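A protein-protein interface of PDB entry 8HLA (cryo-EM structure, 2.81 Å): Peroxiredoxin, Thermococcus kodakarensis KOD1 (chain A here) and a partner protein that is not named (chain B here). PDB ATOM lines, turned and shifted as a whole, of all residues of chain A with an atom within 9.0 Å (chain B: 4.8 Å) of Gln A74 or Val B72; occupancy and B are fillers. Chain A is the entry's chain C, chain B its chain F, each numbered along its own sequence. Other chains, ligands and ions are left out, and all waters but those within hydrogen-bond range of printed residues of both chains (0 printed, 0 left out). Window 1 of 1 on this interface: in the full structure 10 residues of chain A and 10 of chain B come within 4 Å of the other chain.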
ATOM      1  N   LYS A  14      24.401 -14.468  12.572  1.00  0.00           N
ATOM      2  CA  LYS A  14      23.040 -14.521  13.089  1.00  0.00           C
ATOM      3  C   LYS A  14      22.104 -13.860  12.088  1.00  0.00           C
ATOM      4  O   LYS A  14      22.101 -12.637  11.942  1.00  0.00           O
ATOM      5  CB  LYS A  14      22.948 -13.856  14.458  1.00  0.00           C
ATOM      6  CG  LYS A  14      23.692 -12.548  14.578  1.00  0.00           C
ATOM      7  CD  LYS A  14      23.524 -11.956  15.959  1.00  0.00           C
ATOM      8  CE  LYS A  14      22.074 -11.618  16.245  1.00  0.00           C
ATOM      9  NZ  LYS A  14      21.927 -10.864  17.524  1.00  0.00           N
ATOM     10  N   THR A  15      21.300 -14.665  11.412  1.00  0.00           N
ATOM     11  CA  THR A  15      20.370 -14.163  10.422  1.00  0.00           C
ATOM     12  C   THR A  15      19.008 -13.930  11.065  1.00  0.00           C
ATOM     13  O   THR A  15      18.796 -14.191  12.248  1.00  0.00           O
ATOM     14  CB  THR A  15      20.256 -15.143   9.258  1.00  0.00           C
ATOM     15  OG1 THR A  15      19.730 -16.384   9.731  1.00  0.00           O
ATOM     16  CG2 THR A  15      21.619 -15.403   8.678  1.00  0.00           C
ATOM     17  N   THR A  16      18.075 -13.417  10.279  1.00  0.00           N
ATOM     18  CA  THR A  16      16.675 -13.454  10.659  1.00  0.00           C
ATOM     19  C   THR A  16      16.061 -14.808  10.386  1.00  0.00           C
ATOM     20  O   THR A  16      14.838 -14.935  10.378  1.00  0.00           O
ATOM     21  CB  THR A  16      15.883 -12.369   9.930  1.00  0.00           C
ATOM     22  OG1 THR A  16      15.700 -12.745   8.563  1.00  0.00           O
ATOM     23  CG2 THR A  16      16.618 -11.052   9.990  1.00  0.00           C
ATOM     24  N   HIS A  38      24.346  -4.432   2.259  1.00  0.00           N
ATOM     25  CA  HIS A  38      23.933  -3.104   1.939  1.00  0.00           C
ATOM     26  C   HIS A  38      24.493  -2.198   3.013  1.00  0.00           C
ATOM     27  O   HIS A  38      24.622  -2.625   4.165  1.00  0.00           O
ATOM     28  CB  HIS A  38      22.416  -2.957   1.842  1.00  0.00           C
ATOM     29  CG  HIS A  38      21.678  -3.239   3.113  1.00  0.00           C
ATOM     30  ND1 HIS A  38      21.454  -2.280   4.073  1.00  0.00           N
ATOM     31  CD2 HIS A  38      21.063  -4.360   3.554  1.00  0.00           C
ATOM     32  CE1 HIS A  38      20.752  -2.802   5.061  1.00  0.00           C
ATOM     33  NE2 HIS A  38      20.503  -4.065   4.772  1.00  0.00           N
ATOM     34  N   ALA A  40      24.519   0.734   5.811  1.00  0.00           N
ATOM     35  CA  ALA A  40      23.566   1.485   6.616  1.00  0.00           C
ATOM     36  C   ALA A  40      23.755   2.980   6.387  1.00  0.00           C
ATOM     37  O   ALA A  40      23.932   3.776   7.301  1.00  0.00           O
ATOM     38  CB  ALA A  40      23.711   1.111   8.084  1.00  0.00           C
ATOM     39  N   SER A  71      23.969  -6.675   6.682  1.00  0.00           N
ATOM     40  CA  SER A  71      24.342  -5.301   6.986  1.00  0.00           C
ATOM     41  C   SER A  71      24.794  -5.231   8.430  1.00  0.00           C
ATOM     42  O   SER A  71      24.683  -6.195   9.185  1.00  0.00           O
ATOM     43  CB  SER A  71      23.202  -4.318   6.737  1.00  0.00           C
ATOM     44  OG  SER A  71      21.981  -4.830   7.201  1.00  0.00           O
ATOM     45  N   VAL A  72      25.325  -4.073   8.801  1.00  0.00           N
ATOM     46  CA  VAL A  72      25.674  -3.811  10.199  1.00  0.00           C
ATOM     47  C   VAL A  72      24.430  -3.205  10.837  1.00  0.00           C
ATOM     48  O   VAL A  72      24.268  -1.994  10.984  1.00  0.00           O
ATOM     49  CB  VAL A  72      26.930  -2.949  10.333  1.00  0.00           C
ATOM     50  CG1 VAL A  72      28.110  -3.703   9.773  1.00  0.00           C
ATOM     51  CG2 VAL A  72      26.789  -1.666   9.567  1.00  0.00           C
ATOM     52  N   ASP A  73      23.521  -4.089  11.225  1.00  0.00           N
ATOM     53  CA  ASP A  73      22.342  -3.742  11.991  1.00  0.00           C
ATOM     54  C   ASP A  73      22.098  -4.877  12.962  1.00  0.00           C
ATOM     55  O   ASP A  73      22.798  -5.889  12.947  1.00  0.00           O
ATOM     56  CB  ASP A  73      21.114  -3.537  11.111  1.00  0.00           C
ATOM     57  CG  ASP A  73      20.986  -2.130  10.616  1.00  0.00           C
ATOM     58  OD1 ASP A  73      21.515  -1.222  11.282  1.00  0.00           O
ATOM     59  OD2 ASP A  73      20.350  -1.925   9.566  1.00  0.00           O
ATOM     60  N   GLN A  74      21.107  -4.696  13.816  1.00  0.00           N
ATOM     61  CA  GLN A  74      20.609  -5.763  14.663  1.00  0.00           C
ATOM     62  C   GLN A  74      19.285  -6.269  14.132  1.00  0.00           C
ATOM     63  O   GLN A  74      18.562  -5.572  13.422  1.00  0.00           O
ATOM     64  CB  GLN A  74      20.468  -5.301  16.111  1.00  0.00           C
ATOM     65  CG  GLN A  74      21.784  -5.009  16.787  1.00  0.00           C
ATOM     66  CD  GLN A  74      22.310  -3.663  16.438  1.00  0.00           C
ATOM     67  OE1 GLN A  74      21.577  -2.812  15.947  1.00  0.00           O
ATOM     68  NE2 GLN A  74      23.595  -3.454  16.674  1.00  0.00           N
ATOM     69  N   VAL A  75      18.978  -7.508  14.498  1.00  0.00           N
ATOM     70  CA  VAL A  75      17.873  -8.223  13.889  1.00  0.00           C
ATOM     71  C   VAL A  75      16.564  -7.488  14.113  1.00  0.00           C
ATOM     72  O   VAL A  75      15.631  -7.609  13.318  1.00  0.00           O
ATOM     73  CB  VAL A  75      17.833  -9.656  14.449  1.00  0.00           C
ATOM     74  CG1 VAL A  75      16.648 -10.409  13.920  1.00  0.00           C
ATOM     75  CG2 VAL A  75      19.104 -10.383  14.125  1.00  0.00           C
ATOM     76  N   PHE A  76      16.470  -6.711  15.184  1.00  0.00           N
ATOM     77  CA  PHE A  76      15.199  -6.088  15.522  1.00  0.00           C
ATOM     78  C   PHE A  76      14.876  -4.937  14.589  1.00  0.00           C
ATOM     79  O   PHE A  76      13.726  -4.770  14.181  1.00  0.00           O
ATOM     80  CB  PHE A  76      15.225  -5.636  16.976  1.00  0.00           C
ATOM     81  CG  PHE A  76      15.937  -6.585  17.874  1.00  0.00           C
ATOM     82  CD1 PHE A  76      15.320  -7.741  18.295  1.00  0.00           C
ATOM     83  CD2 PHE A  76      17.237  -6.344  18.265  1.00  0.00           C
ATOM     84  CE1 PHE A  76      15.977  -8.624  19.106  1.00  0.00           C
ATOM     85  CE2 PHE A  76      17.900  -7.228  19.076  1.00  0.00           C
ATOM     86  CZ  PHE A  76      17.268  -8.369  19.499  1.00  0.00           C
ATOM     87  N   SER A  77      15.872  -4.131  14.234  1.00  0.00           N
ATOM     88  CA  SER A  77      15.626  -3.078  13.259  1.00  0.00           C
ATOM     89  C   SER A  77      15.419  -3.650  11.868  1.00  0.00           C
ATOM     90  O   SER A  77      14.631  -3.111  11.091  1.00  0.00           O
ATOM     91  CB  SER A  77      16.768  -2.078  13.262  1.00  0.00           C
ATOM     92  OG  SER A  77      16.614  -1.180  14.332  1.00  0.00           O
ATOM     93  N   HIS A  78      16.115  -4.734  11.532  1.00  0.00           N
ATOM     94  CA  HIS A  78      15.891  -5.383  10.248  1.00  0.00           C
ATOM     95  C   HIS A  78      14.476  -5.904  10.128  1.00  0.00           C
ATOM     96  O   HIS A  78      13.772  -5.586   9.167  1.00  0.00           O
ATOM     97  CB  HIS A  78      16.870  -6.526  10.058  1.00  0.00           C
ATOM     98  CG  HIS A  78      18.150  -6.114   9.424  1.00  0.00           C
ATOM     99  ND1 HIS A  78      19.350  -6.717   9.727  1.00  0.00           N
ATOM    100  CD2 HIS A  78      18.420  -5.174   8.490  1.00  0.00           C
ATOM    101  CE1 HIS A  78      20.311  -6.148   9.024  1.00  0.00           C
ATOM    102  NE2 HIS A  78      19.773  -5.211   8.263  1.00  0.00           N
ATOM    103  N   ILE A  79      14.033  -6.705  11.096  1.00  0.00           N
ATOM    104  CA  ILE A  79      12.709  -7.300  10.995  1.00  0.00           C
ATOM    105  C   ILE A  79      11.651  -6.218  10.969  1.00  0.00           C
ATOM    106  O   ILE A  79      10.690  -6.289  10.201  1.00  0.00           O
ATOM    107  CB  ILE A  79      12.463  -8.293  12.139  1.00  0.00           C
ATOM    108  CG1 ILE A  79      13.458  -9.432  12.083  1.00  0.00           C
ATOM    109  CG2 ILE A  79      11.080  -8.863  12.037  1.00  0.00           C
ATOM    110  CD1 ILE A  79      13.254 -10.413  13.175  1.00  0.00           C
ATOM    111  N   LYS A  80      11.810  -5.197  11.798  1.00  0.00           N
ATOM    112  CA  LYS A  80      10.871  -4.090  11.787  1.00  0.00           C
ATOM    113  C   LYS A  80      10.926  -3.338  10.467  1.00  0.00           C
ATOM    114  O   LYS A  80       9.896  -2.878   9.971  1.00  0.00           O
ATOM    115  CB  LYS A  80      11.163  -3.180  12.977  1.00  0.00           C
ATOM    116  CG  LYS A  80      10.145  -2.103  13.236  1.00  0.00           C
ATOM    117  CD  LYS A  80       8.738  -2.629  13.287  1.00  0.00           C
ATOM    118  CE  LYS A  80       8.430  -3.268  14.592  1.00  0.00           C
ATOM    119  NZ  LYS A  80       6.969  -3.395  14.741  1.00  0.00           N
ATOM    120  N   TRP A  81      12.121  -3.204   9.896  1.00  0.00           N
ATOM    121  CA  TRP A  81      12.280  -2.675   8.546  1.00  0.00           C
ATOM    122  C   TRP A  81      11.600  -3.561   7.514  1.00  0.00           C
ATOM    123  O   TRP A  81      10.903  -3.069   6.624  1.00  0.00           O
ATOM    124  CB  TRP A  81      13.765  -2.546   8.262  1.00  0.00           C
ATOM    125  CG  TRP A  81      14.183  -1.906   7.002  1.00  0.00           C
ATOM    126  CD1 TRP A  81      13.400  -1.434   6.004  1.00  0.00           C
ATOM    127  CD2 TRP A  81      15.526  -1.692   6.599  1.00  0.00           C
ATOM    128  NE1 TRP A  81      14.176  -0.931   4.999  1.00  0.00           N
ATOM    129  CE2 TRP A  81      15.491  -1.077   5.345  1.00  0.00           C
ATOM    130  CE3 TRP A  81      16.763  -1.954   7.189  1.00  0.00           C
ATOM    131  CZ2 TRP A  81      16.644  -0.739   4.655  1.00  0.00           C
ATOM    132  CZ3 TRP A  81      17.907  -1.602   6.513  1.00  0.00           C
ATOM    133  CH2 TRP A  81      17.842  -0.994   5.261  1.00  0.00           C
ATOM    134  N   MET A  82      11.796  -4.872   7.608  1.00  0.00           N
ATOM    135  CA  MET A  82      11.121  -5.777   6.690  1.00  0.00           C
ATOM    136  C   MET A  82       9.627  -5.849   6.962  1.00  0.00           C
ATOM    137  O   MET A  82       8.852  -6.127   6.045  1.00  0.00           O
ATOM    138  CB  MET A  82      11.757  -7.159   6.759  1.00  0.00           C
ATOM    139  CG  MET A  82      13.232  -7.144   6.431  1.00  0.00           C
ATOM    140  SD  MET A  82      13.549  -6.131   4.976  1.00  0.00           S
ATOM    141  CE  MET A  82      15.076  -5.320   5.401  1.00  0.00           C
ATOM    142  N   VAL A  97      18.757 -12.480   6.588  1.00  0.00           N
ATOM    143  CA  VAL A  97      19.567 -11.271   6.583  1.00  0.00           C
ATOM    144  C   VAL A  97      20.533 -11.367   7.753  1.00  0.00           C
ATOM    145  O   VAL A  97      20.102 -11.349   8.907  1.00  0.00           O
ATOM    146  CB  VAL A  97      18.727  -9.992   6.696  1.00  0.00           C
ATOM    147  CG1 VAL A  97      19.624  -8.791   6.704  1.00  0.00           C
ATOM    148  CG2 VAL A  97      17.746  -9.885   5.566  1.00  0.00           C
ATOM    149  N   ILE A  98      21.834 -11.459   7.469  1.00  0.00           N
ATOM    150  CA  ILE A  98      22.808 -11.421   8.548  1.00  0.00           C
ATOM    151  C   ILE A  98      22.750 -10.066   9.229  1.00  0.00           C
ATOM    152  O   ILE A  98      22.718  -9.020   8.573  1.00  0.00           O
ATOM    153  CB  ILE A  98      24.235 -11.705   8.057  1.00  0.00           C
ATOM    154  CG1 ILE A  98      24.393 -13.109   7.506  1.00  0.00           C
ATOM    155  CG2 ILE A  98      25.239 -11.492   9.164  1.00  0.00           C
ATOM    156  CD1 ILE A  98      24.159 -13.218   6.095  1.00  0.00           C
ATOM    157  N   ALA A  99      22.740 -10.079  10.555  1.00  0.00           N
ATOM    158  CA  ALA A  99      22.782  -8.857  11.347  1.00  0.00           C
ATOM    159  C   ALA A  99      24.156  -8.637  11.951  1.00  0.00           C
ATOM    160  O   ALA A  99      24.279  -8.237  13.108  1.00  0.00           O
ATOM    161  CB  ALA A  99      21.713  -8.891  12.424  1.00  0.00           C
ATOM    162  N   ASP A 100      25.199  -8.920  11.178  1.00  0.00           N
ATOM    163  CA  ASP A 100      26.575  -8.758  11.624  1.00  0.00           C
ATOM    164  C   ASP A 100      26.816  -7.361  12.160  1.00  0.00           C
ATOM    165  O   ASP A 100      26.780  -6.386  11.409  1.00  0.00           O
ATOM    166  CB  ASP A 100      27.526  -9.030  10.458  1.00  0.00           C
ATOM    167  CG  ASP A 100      28.968  -9.183  10.900  1.00  0.00           C
ATOM    168  OD1 ASP A 100      29.227  -9.244  12.122  1.00  0.00           O
ATOM    169  OD2 ASP A 100      29.851  -9.222  10.018  1.00  0.00           O
ATOM    170  N   ASP A 101      27.086  -7.271  13.453  1.00  0.00           N
ATOM    171  CA  ASP A 101      27.451  -6.024  14.103  1.00  0.00           C
ATOM    172  C   ASP A 101      28.961  -5.964  14.271  1.00  0.00           C
ATOM    173  O   ASP A 101      29.615  -7.001  14.439  1.00  0.00           O
ATOM    174  CB  ASP A 101      26.750  -5.887  15.455  1.00  0.00           C
ATOM    175  CG  ASP A 101      26.988  -7.079  16.363  1.00  0.00           C
ATOM    176  OD1 ASP A 101      27.599  -8.071  15.907  1.00  0.00           O
ATOM    177  OD2 ASP A 101      26.583  -7.017  17.544  1.00  0.00           O
ATOM    178  N   ARG A 102      29.511  -4.751  14.216  1.00  0.00           N
ATOM    179  CA  ARG A 102      30.955  -4.561  14.139  1.00  0.00           C
ATOM    180  C   ARG A 102      31.516  -5.453  13.030  1.00  0.00           C
ATOM    181  O   ARG A 102      32.243  -6.419  13.266  1.00  0.00           O
ATOM    182  CB  ARG A 102      31.611  -4.841  15.497  1.00  0.00           C
ATOM    183  CG  ARG A 102      33.115  -4.628  15.550  1.00  0.00           C
ATOM    184  CD  ARG A 102      33.478  -3.161  15.476  1.00  0.00           C
ATOM    185  NE  ARG A 102      34.924  -2.955  15.436  1.00  0.00           N
ATOM    186  CZ  ARG A 102      35.682  -2.793  16.514  1.00  0.00           C
ATOM    187  NH1 ARG A 102      35.129  -2.817  17.717  1.00  0.00           N
ATOM    188  NH2 ARG A 102      36.989  -2.611  16.394  1.00  0.00           N
ATOM    189  N   PRO B  39      21.056  -1.222  24.443  1.00  0.00           N
ATOM    190  CA  PRO B  39      21.665  -2.139  23.465  1.00  0.00           C
ATOM    191  C   PRO B  39      21.245  -1.886  22.030  1.00  0.00           C
ATOM    192  O   PRO B  39      22.103  -1.702  21.161  1.00  0.00           O
ATOM    193  CB  PRO B  39      21.202  -3.513  23.959  1.00  0.00           C
ATOM    194  CG  PRO B  39      20.807  -3.309  25.351  1.00  0.00           C
ATOM    195  CD  PRO B  39      20.236  -1.953  25.411  1.00  0.00           C
ATOM    196  N   ALA B  40      19.946  -1.862  21.752  1.00  0.00           N
ATOM    197  CA  ALA B  40      19.468  -1.754  20.386  1.00  0.00           C
ATOM    198  C   ALA B  40      18.133  -1.034  20.370  1.00  0.00           C
ATOM    199  O   ALA B  40      17.419  -0.994  21.369  1.00  0.00           O
ATOM    200  CB  ALA B  40      19.326  -3.132  19.740  1.00  0.00           C
ATOM    201  N   LEU B  70      22.134   6.651  23.506  1.00  0.00           N
ATOM    202  CA  LEU B  70      23.183   6.153  22.638  1.00  0.00           C
ATOM    203  C   LEU B  70      22.898   4.696  22.339  1.00  0.00           C
ATOM    204  O   LEU B  70      22.422   3.968  23.203  1.00  0.00           O
ATOM    205  CB  LEU B  70      24.566   6.297  23.275  1.00  0.00           C
ATOM    206  CG  LEU B  70      25.777   5.825  22.471  1.00  0.00           C
ATOM    207  CD1 LEU B  70      26.943   6.717  22.738  1.00  0.00           C
ATOM    208  CD2 LEU B  70      26.151   4.407  22.794  1.00  0.00           C
ATOM    209  N   SER B  71      23.172   4.283  21.111  1.00  0.00           N
ATOM    210  CA  SER B  71      23.250   2.861  20.820  1.00  0.00           C
ATOM    211  C   SER B  71      24.043   2.694  19.543  1.00  0.00           C
ATOM    212  O   SER B  71      24.237   3.649  18.793  1.00  0.00           O
ATOM    213  CB  SER B  71      21.870   2.205  20.710  1.00  0.00           C
ATOM    214  OG  SER B  71      21.163   2.642  19.575  1.00  0.00           O
ATOM    215  N   VAL B  72      24.521   1.479  19.308  1.00  0.00           N
ATOM    216  CA  VAL B  72      25.234   1.186  18.062  1.00  0.00           C
ATOM    217  C   VAL B  72      24.158   0.790  17.065  1.00  0.00           C
ATOM    218  O   VAL B  72      24.003  -0.367  16.677  1.00  0.00           O
ATOM    219  CB  VAL B  72      26.306   0.110  18.244  1.00  0.00           C
ATOM    220  CG1 VAL B  72      27.476   0.680  18.990  1.00  0.00           C
ATOM    221  CG2 VAL B  72      25.751  -1.084  18.985  1.00  0.00           C
ATOM    222  N   ASP B  73      23.450   1.797  16.577  1.00  0.00           N
ATOM    223  CA  ASP B  73      22.424   1.629  15.572  1.00  0.00           C
ATOM    224  C   ASP B  73      22.599   2.770  14.594  1.00  0.00           C
ATOM    225  O   ASP B  73      23.600   3.485  14.626  1.00  0.00           O
ATOM    226  CB  ASP B  73      21.011   1.640  16.162  1.00  0.00           C
ATOM    227  CG  ASP B  73      20.574   0.288  16.662  1.00  0.00           C
ATOM    228  OD1 ASP B  73      21.441  -0.509  17.031  1.00  0.00           O
ATOM    229  OD2 ASP B  73      19.364   0.032  16.757  1.00  0.00           O
ATOM    230  N   GLN B  74      21.620   2.945  13.727  1.00  0.00           N
ATOM    231  CA  GLN B  74      21.615   4.027  12.766  1.00  0.00           C
ATOM    232  C   GLN B  74      20.554   5.028  13.171  1.00  0.00           C
ATOM    233  O   GLN B  74      19.508   4.656  13.699  1.00  0.00           O
ATOM    234  CB  GLN B  74      21.333   3.503  11.362  1.00  0.00           C
ATOM    235  CG  GLN B  74      22.415   2.619  10.818  1.00  0.00           C
ATOM    236  CD  GLN B  74      23.794   3.181  11.041  1.00  0.00           C
ATOM    237  OE1 GLN B  74      24.045   4.347  10.762  1.00  0.00           O
ATOM    238  NE2 GLN B  74      24.703   2.353  11.529  1.00  0.00           N
ATOM    239  N   ASP B 100      26.528   5.594  17.063  1.00  0.00           N
ATOM    240  CA  ASP B 100      27.954   5.526  16.785  1.00  0.00           C
ATOM    241  C   ASP B 100      28.248   4.359  15.854  1.00  0.00           C
ATOM    242  O   ASP B 100      27.667   3.278  15.982  1.00  0.00           O
ATOM    243  CB  ASP B 100      28.785   5.413  18.063  1.00  0.00           C
ATOM    244  CG  ASP B 100      28.295   4.348  18.976  1.00  0.00           C
ATOM    245  OD1 ASP B 100      27.160   3.878  18.771  1.00  0.00           O
ATOM    246  OD2 ASP B 100      29.043   3.982  19.900  1.00  0.00           O
ATOM    247  N   ARG B 102      29.742   1.330  14.541  1.00  0.00           N
ATOM    248  CA  ARG B 102      30.456   0.165  15.060  1.00  0.00           C
ATOM    249  C   ARG B 102      31.108   0.481  16.402  1.00  0.00           C
ATOM    250  O   ARG B 102      32.188  -0.015  16.729  1.00  0.00           O
ATOM    251  CB  ARG B 102      31.485  -0.351  14.049  1.00  0.00           C
ATOM    252  CG  ARG B 102      30.864  -1.101  12.875  1.00  0.00           C
ATOM    253  CD  ARG B 102      31.890  -1.542  11.834  1.00  0.00           C
ATOM    254  NE  ARG B 102      32.782  -2.590  12.316  1.00  0.00           N
ATOM    255  CZ  ARG B 102      33.782  -3.106  11.611  1.00  0.00           C
ATOM    256  NH1 ARG B 102      34.024  -2.674  10.381  1.00  0.00           N
ATOM    257  NH2 ARG B 102      34.538  -4.060  12.135  1.00  0.00           N
ATOM    258  N   GLY B 103      30.447   1.344  17.170  1.00  0.00           N
ATOM    259  CA  GLY B 103      30.837   1.652  18.528  1.00  0.00           C
ATOM    260  C   GLY B 103      32.234   2.187  18.728  1.00  0.00           C
ATOM    261  O   GLY B 103      33.093   1.478  19.250  1.00  0.00           O
ATOM    262  N   ALA B 106      31.222   4.106  22.261  1.00  0.00           N
ATOM    263  CA  ALA B 106      30.877   3.048  23.198  1.00  0.00           C
ATOM    264  C   ALA B 106      32.097   2.248  23.614  1.00  0.00           C
ATOM    265  O   ALA B 106      32.229   1.870  24.780  1.00  0.00           O
ATOM    266  CB  ALA B 106      29.835   2.129  22.578  1.00  0.00           C
ATOM    267  N   THR B 117      29.732  -7.000  21.006  1.00  0.00           N
ATOM    268  CA  THR B 117      29.965  -5.871  20.121  1.00  0.00           C
ATOM    269  C   THR B 117      28.843  -4.846  20.176  1.00  0.00           C
ATOM    270  O   THR B 117      28.906  -3.837  19.471  1.00  0.00           O
ATOM    271  CB  THR B 117      30.148  -6.364  18.681  1.00  0.00           C
ATOM    272  OG1 THR B 117      29.032  -7.177  18.319  1.00  0.00           O
ATOM    273  CG2 THR B 117      31.409  -7.191  18.553  1.00  0.00           C
ATOM    274  N   ILE B 118      27.829  -5.085  20.989  1.00  0.00           N
ATOM    275  CA  ILE B 118      26.738  -4.164  21.224  1.00  0.00           C
ATOM    276  C   ILE B 118      26.962  -3.533  22.594  1.00  0.00           C
ATOM    277  O   ILE B 118      27.813  -3.969  23.369  1.00  0.00           O
ATOM    278  CB  ILE B 118      25.394  -4.924  21.139  1.00  0.00           C
ATOM    279  CG1 ILE B 118      24.230  -4.009  20.834  1.00  0.00           C
ATOM    280  CG2 ILE B 118      25.111  -5.675  22.413  1.00  0.00           C
ATOM    281  CD1 ILE B 118      22.936  -4.769  20.800  1.00  0.00           C
ATOM    282  N   THR B 119      26.217  -2.481  22.905  1.00  0.00           N
ATOM    283  CA  THR B 119      26.386  -1.884  24.221  1.00  0.00           C
ATOM    284  C   THR B 119      25.485  -2.546  25.259  1.00  0.00           C
ATOM    285  O   THR B 119      24.516  -3.238  24.938  1.00  0.00           O
ATOM    286  CB  THR B 119      26.100  -0.386  24.207  1.00  0.00           C
ATOM    287  OG1 THR B 119      24.756  -0.153  23.783  1.00  0.00           O
ATOM    288  CG2 THR B 119      27.020   0.319  23.297  1.00  0.00           C
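The backbone carbonyl oxygen (O) of Arg A102 lies close to the guanidinium group (NH2) of Arg B102, 3.5 Å away. The side-chain hydroxyl (OG1) of Thr B117 lies within hydrogen-bond range of the side-chain carboxylate (OD2) of Asp A101 (2.6 Å). NE2 of Gln A74 sits at hydrogen-bond distance from O of Val B72 (3.1 Å). The side-chain carboxylate of Asp B73 sits close to the side-chain amide oxygen of Gln A74.
Among the printed residues, pairs that only touch across the chains: Ala A40 with Gln B74 (3.4 Å), Asp A73 with Gln B74 (3.97 Å), Ser A77 with Asp B73 (3.9 Å) and Arg A102 with Thr B117 (3.8 Å).
Gln A74 touches just these residues of chain B: Val B72 (3.1 Å) and Asp B73 (2.5 Å). No residue of chain A comes within 4 Å of Ser B71. Of the printed residues of chain A, Gln B74 touches Ala A40 (3.4 Å) and Asp A73 (3.97 Å). Of the printed residues of chain B, Ser A77 touches Asp B73. Lys A14 touches none of the printed residues of chain B. Thr A16 touches none of the printed residues of chain B.
Of the 23 printed residues of chain A, 6 touch a printed residue of chain B. Hydrophobic or aromatic side chains of chain A within 4 Å of the printed part of chain B: Ala A40. Of the 14 printed residues of chain B, 5 touch a printed residue of chain A. Among the printed residues, 8 pairs touch across the chains. Among the printed residues, no Asp or Glu carboxylate lies within 4 Å of a Lys or Arg side-chain nitrogen of the other chain.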
